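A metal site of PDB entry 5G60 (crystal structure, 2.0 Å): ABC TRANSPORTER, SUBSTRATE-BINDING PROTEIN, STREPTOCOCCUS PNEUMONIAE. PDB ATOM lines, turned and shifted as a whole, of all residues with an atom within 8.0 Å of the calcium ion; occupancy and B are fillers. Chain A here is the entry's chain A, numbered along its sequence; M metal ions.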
ATOM      1  N   TRP A 145      -1.448 -19.071 -21.709  1.00  0.00           N
ATOM      2  CA  TRP A 145      -1.581 -20.487 -21.956  1.00  0.00           C
ATOM      3  C   TRP A 145      -3.001 -20.947 -21.971  1.00  0.00           C
ATOM      4  O   TRP A 145      -3.373 -21.770 -22.832  1.00  0.00           O
ATOM      5  CB  TRP A 145      -0.791 -21.304 -20.952  1.00  0.00           C
ATOM      6  CG  TRP A 145       0.646 -21.034 -21.065  1.00  0.00           C
ATOM      7  CD1 TRP A 145       1.279 -20.202 -21.979  1.00  0.00           C
ATOM      8  CD2 TRP A 145       1.657 -21.604 -20.272  1.00  0.00           C
ATOM      9  NE1 TRP A 145       2.606 -20.198 -21.745  1.00  0.00           N
ATOM     10  CE2 TRP A 145       2.886 -21.058 -20.717  1.00  0.00           C
ATOM     11  CE3 TRP A 145       1.666 -22.521 -19.225  1.00  0.00           C
ATOM     12  CZ2 TRP A 145       4.107 -21.404 -20.138  1.00  0.00           C
ATOM     13  CZ3 TRP A 145       2.875 -22.870 -18.652  1.00  0.00           C
ATOM     14  CH2 TRP A 145       4.072 -22.317 -19.101  1.00  0.00           C
ATOM     15  N   PHE A 167      -1.133 -27.913 -19.399  1.00  0.00           N
ATOM     16  CA  PHE A 167       0.099 -27.133 -19.477  1.00  0.00           C
ATOM     17  C   PHE A 167       1.284 -28.077 -19.698  1.00  0.00           C
ATOM     18  O   PHE A 167       2.133 -27.864 -20.590  1.00  0.00           O
ATOM     19  CB  PHE A 167       0.300 -26.272 -18.201  1.00  0.00           C
ATOM     20  CG  PHE A 167      -0.671 -25.098 -18.026  1.00  0.00           C
ATOM     21  CD1 PHE A 167      -1.595 -24.711 -18.999  1.00  0.00           C
ATOM     22  CD2 PHE A 167      -0.631 -24.366 -16.836  1.00  0.00           C
ATOM     23  CE1 PHE A 167      -2.413 -23.599 -18.806  1.00  0.00           C
ATOM     24  CE2 PHE A 167      -1.438 -23.273 -16.642  1.00  0.00           C
ATOM     25  CZ  PHE A 167      -2.342 -22.884 -17.620  1.00  0.00           C
ATOM     26  N   LYS A 168       1.335 -29.137 -18.913  1.00  0.00           N
ATOM     27  CA  LYS A 168       2.425 -30.066 -19.017  1.00  0.00           C
ATOM     28  C   LYS A 168       2.597 -30.659 -20.433  1.00  0.00           C
ATOM     29  O   LYS A 168       3.719 -30.735 -20.944  1.00  0.00           O
ATOM     30  CB  LYS A 168       2.233 -31.223 -18.073  1.00  0.00           C
ATOM     31  CG  LYS A 168       3.529 -31.934 -17.986  1.00  0.00           C
ATOM     32  CD  LYS A 168       3.452 -33.197 -17.215  1.00  0.00           C
ATOM     33  CE  LYS A 168       4.875 -33.705 -17.114  1.00  0.00           C
ATOM     34  NZ  LYS A 168       4.802 -35.088 -16.664  1.00  0.00           N
ATOM     35  N   ASN A 169       1.493 -31.102 -21.009  1.00  0.00           N
ATOM     36  CA  ASN A 169       1.497 -31.924 -22.210  1.00  0.00           C
ATOM     37  C   ASN A 169       1.088 -31.169 -23.466  1.00  0.00           C
ATOM     38  O   ASN A 169       1.370 -31.629 -24.560  1.00  0.00           O
ATOM     39  CB  ASN A 169       0.523 -33.083 -22.020  1.00  0.00           C
ATOM     40  CG  ASN A 169       0.902 -33.976 -20.861  1.00  0.00           C
ATOM     41  OD1 ASN A 169       2.090 -34.257 -20.586  1.00  0.00           O
ATOM     42  ND2 ASN A 169      -0.129 -34.478 -20.170  1.00  0.00           N
ATOM     43  N   GLY A 170       0.403 -30.030 -23.314  1.00  0.00           N
ATOM     44  CA  GLY A 170      -0.238 -29.371 -24.413  1.00  0.00           C
ATOM     45  C   GLY A 170       0.628 -28.384 -25.159  1.00  0.00           C
ATOM     46  O   GLY A 170       0.154 -27.798 -26.114  1.00  0.00           O
ATOM     47  N   ASP A 171       1.899 -28.184 -24.746  1.00  0.00           N
ATOM     48  CA  ASP A 171       2.776 -27.199 -25.410  1.00  0.00           C
ATOM     49  C   ASP A 171       2.104 -25.850 -25.630  1.00  0.00           C
ATOM     50  O   ASP A 171       1.991 -25.379 -26.733  1.00  0.00           O
ATOM     51  CB  ASP A 171       3.346 -27.768 -26.731  1.00  0.00           C
ATOM     52  CG  ASP A 171       4.455 -26.907 -27.328  1.00  0.00           C
ATOM     53  OD1 ASP A 171       5.196 -26.268 -26.558  1.00  0.00           O
ATOM     54  OD2 ASP A 171       4.569 -26.849 -28.558  1.00  0.00           O
ATOM     55  N   PRO A 172       1.653 -25.196 -24.550  1.00  0.00           N
ATOM     56  CA  PRO A 172       0.965 -23.953 -24.773  1.00  0.00           C
ATOM     57  C   PRO A 172       1.835 -22.843 -25.284  1.00  0.00           C
ATOM     58  O   PRO A 172       1.315 -21.986 -26.007  1.00  0.00           O
ATOM     59  CB  PRO A 172       0.362 -23.622 -23.396  1.00  0.00           C
ATOM     60  CG  PRO A 172       1.197 -24.342 -22.437  1.00  0.00           C
ATOM     61  CD  PRO A 172       1.543 -25.618 -23.148  1.00  0.00           C
ATOM     62  N   ASN A 173       3.108 -22.790 -24.932  1.00  0.00           N
ATOM     63  CA  ASN A 173       3.979 -21.772 -25.538  1.00  0.00           C
ATOM     64  C   ASN A 173       4.412 -22.079 -27.005  1.00  0.00           C
ATOM     65  O   ASN A 173       5.062 -21.264 -27.622  1.00  0.00           O
ATOM     66  CB  ASN A 173       5.190 -21.396 -24.655  1.00  0.00           C
ATOM     67  CG  ASN A 173       6.255 -22.475 -24.536  1.00  0.00           C
ATOM     68  OD1 ASN A 173       6.245 -23.517 -25.214  1.00  0.00           O
ATOM     69  ND2 ASN A 173       7.232 -22.206 -23.695  1.00  0.00           N
ATOM     70  N   GLY A 174       4.096 -23.281 -27.502  1.00  0.00           N
ATOM     71  CA  GLY A 174       4.167 -23.567 -28.924  1.00  0.00           C
ATOM     72  C   GLY A 174       5.576 -23.565 -29.505  1.00  0.00           C
ATOM     73  O   GLY A 174       5.824 -22.968 -30.550  1.00  0.00           O
ATOM     74  N   ASN A 175       6.486 -24.224 -28.835  1.00  0.00           N
ATOM     75  CA  ASN A 175       7.856 -24.350 -29.322  1.00  0.00           C
ATOM     76  C   ASN A 175       8.276 -25.828 -29.526  1.00  0.00           C
ATOM     77  O   ASN A 175       9.467 -26.128 -29.628  1.00  0.00           O
ATOM     78  CB  ASN A 175       8.792 -23.611 -28.382  1.00  0.00           C
ATOM     79  CG  ASN A 175       8.787 -24.132 -26.919  1.00  0.00           C
ATOM     80  OD1 ASN A 175       8.111 -25.118 -26.508  1.00  0.00           O
ATOM     81  ND2 ASN A 175       9.585 -23.450 -26.121  1.00  0.00           N
ATOM     82  N   GLY A 176       7.291 -26.713 -29.590  1.00  0.00           N
ATOM     83  CA  GLY A 176       7.497 -28.166 -29.661  1.00  0.00           C
ATOM     84  C   GLY A 176       8.325 -28.793 -28.553  1.00  0.00           C
ATOM     85  O   GLY A 176       8.767 -29.943 -28.726  1.00  0.00           O
ATOM     86  N   GLU A 177       8.533 -28.068 -27.436  1.00  0.00           N
ATOM     87  CA  GLU A 177       9.323 -28.556 -26.289  1.00  0.00           C
ATOM     88  C   GLU A 177       8.444 -28.670 -25.063  1.00  0.00           C
ATOM     89  O   GLU A 177       7.511 -27.876 -24.901  1.00  0.00           O
ATOM     90  CB  GLU A 177      10.504 -27.638 -25.985  1.00  0.00           C
ATOM     91  N   ALA A 178       8.745 -29.638 -24.215  1.00  0.00           N
ATOM     92  CA  ALA A 178       8.083 -29.849 -22.935  1.00  0.00           C
ATOM     93  C   ALA A 178       8.782 -28.978 -21.925  1.00  0.00           C
ATOM     94  O   ALA A 178       9.257 -29.469 -20.910  1.00  0.00           O
ATOM     95  CB  ALA A 178       8.169 -31.307 -22.487  1.00  0.00           C
ATOM     96  N   ASP A 179       8.827 -27.682 -22.188  1.00  0.00           N
ATOM     97  CA  ASP A 179       9.564 -26.759 -21.338  1.00  0.00           C
ATOM     98  C   ASP A 179       8.614 -26.153 -20.269  1.00  0.00           C
ATOM     99  O   ASP A 179       9.072 -25.483 -19.350  1.00  0.00           O
ATOM    100  CB  ASP A 179      10.258 -25.664 -22.162  1.00  0.00           C
ATOM    101  CG  ASP A 179       9.324 -24.852 -22.927  1.00  0.00           C
ATOM    102  OD1 ASP A 179       8.332 -25.409 -23.419  1.00  0.00           O
ATOM    103  OD2 ASP A 179       9.526 -23.651 -23.090  1.00  0.00           O
ATOM    104  N   GLU A 180       7.306 -26.424 -20.369  1.00  0.00           N
ATOM    105  CA  GLU A 180       6.340 -25.829 -19.441  1.00  0.00           C
ATOM    106  C   GLU A 180       6.524 -26.440 -18.067  1.00  0.00           C
ATOM    107  O   GLU A 180       6.576 -27.670 -17.930  1.00  0.00           O
ATOM    108  CB  GLU A 180       4.916 -26.007 -19.957  1.00  0.00           C
ATOM    109  CG  GLU A 180       4.582 -25.123 -21.179  1.00  0.00           C
ATOM    110  CD  GLU A 180       5.011 -25.676 -22.595  1.00  0.00           C
ATOM    111  OE1 GLU A 180       5.738 -26.679 -22.759  1.00  0.00           O
ATOM    112  OE2 GLU A 180       4.654 -25.028 -23.605  1.00  0.00           O
ATOM    113  N   ILE A 181       6.727 -25.583 -17.054  1.00  0.00           N
ATOM    114  CA  ILE A 181       6.735 -26.009 -15.639  1.00  0.00           C
ATOM    115  C   ILE A 181       5.318 -25.703 -15.099  1.00  0.00           C
ATOM    116  O   ILE A 181       4.969 -24.510 -14.918  1.00  0.00           O
ATOM    117  CB  ILE A 181       7.789 -25.222 -14.868  1.00  0.00           C
ATOM    118  CG1 ILE A 181       9.179 -25.413 -15.525  1.00  0.00           C
ATOM    119  CG2 ILE A 181       7.777 -25.588 -13.399  1.00  0.00           C
ATOM    120  CD1 ILE A 181      10.278 -24.504 -15.029  1.00  0.00           C
ATOM    121  N   LYS A 263       8.174 -19.612 -17.939  1.00  0.00           N
ATOM    122  CA  LYS A 263       8.064 -21.067 -17.950  1.00  0.00           C
ATOM    123  C   LYS A 263       6.969 -21.591 -17.036  1.00  0.00           C
ATOM    124  O   LYS A 263       6.685 -22.778 -17.099  1.00  0.00           O
ATOM    125  CB  LYS A 263       9.368 -21.690 -17.505  1.00  0.00           C
ATOM    126  CG  LYS A 263      10.565 -21.302 -18.338  1.00  0.00           C
ATOM    127  CD  LYS A 263      10.446 -21.822 -19.740  1.00  0.00           C
ATOM    128  CE  LYS A 263      11.816 -21.837 -20.434  1.00  0.00           C
ATOM    129  NZ  LYS A 263      11.598 -21.937 -21.891  1.00  0.00           N
HETATM  130 CA    CA M   1       6.577 -25.761 -24.817  1.00  0.00          CA
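OD2 of Asp 179 lies within salt-bridge range of NZ of Lys 263 (2.9 Å). The side-chain carboxylate of Asp 171 sits close to the backbone NH of Gly 174, 3.3 Å away. OD2 of Asp 171 lies within hydrogen-bond range of N of Gly 176 (2.9 Å).
The calcium ion is bound by OD1 of Asp 179 (2.3 Å). The calcium ion is bound by OD1 of Asp 171 (2.3 Å). The side-chain amide oxygen (OD1) of Asn 173 binds the calcium ion. The backbone carbonyl oxygen (O) of Glu 177 is bound to the calcium ion, 2.3 Å away. OD1 of Asn 175 binds the calcium ion, 2.4 Å away. OE2 of Glu 180 is bound to the calcium ion, at 2.4 Å. The calcium ion is bound by OE1 of Glu 180 (2.4 Å). The calcium ion has seven donor atoms within binding distance.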
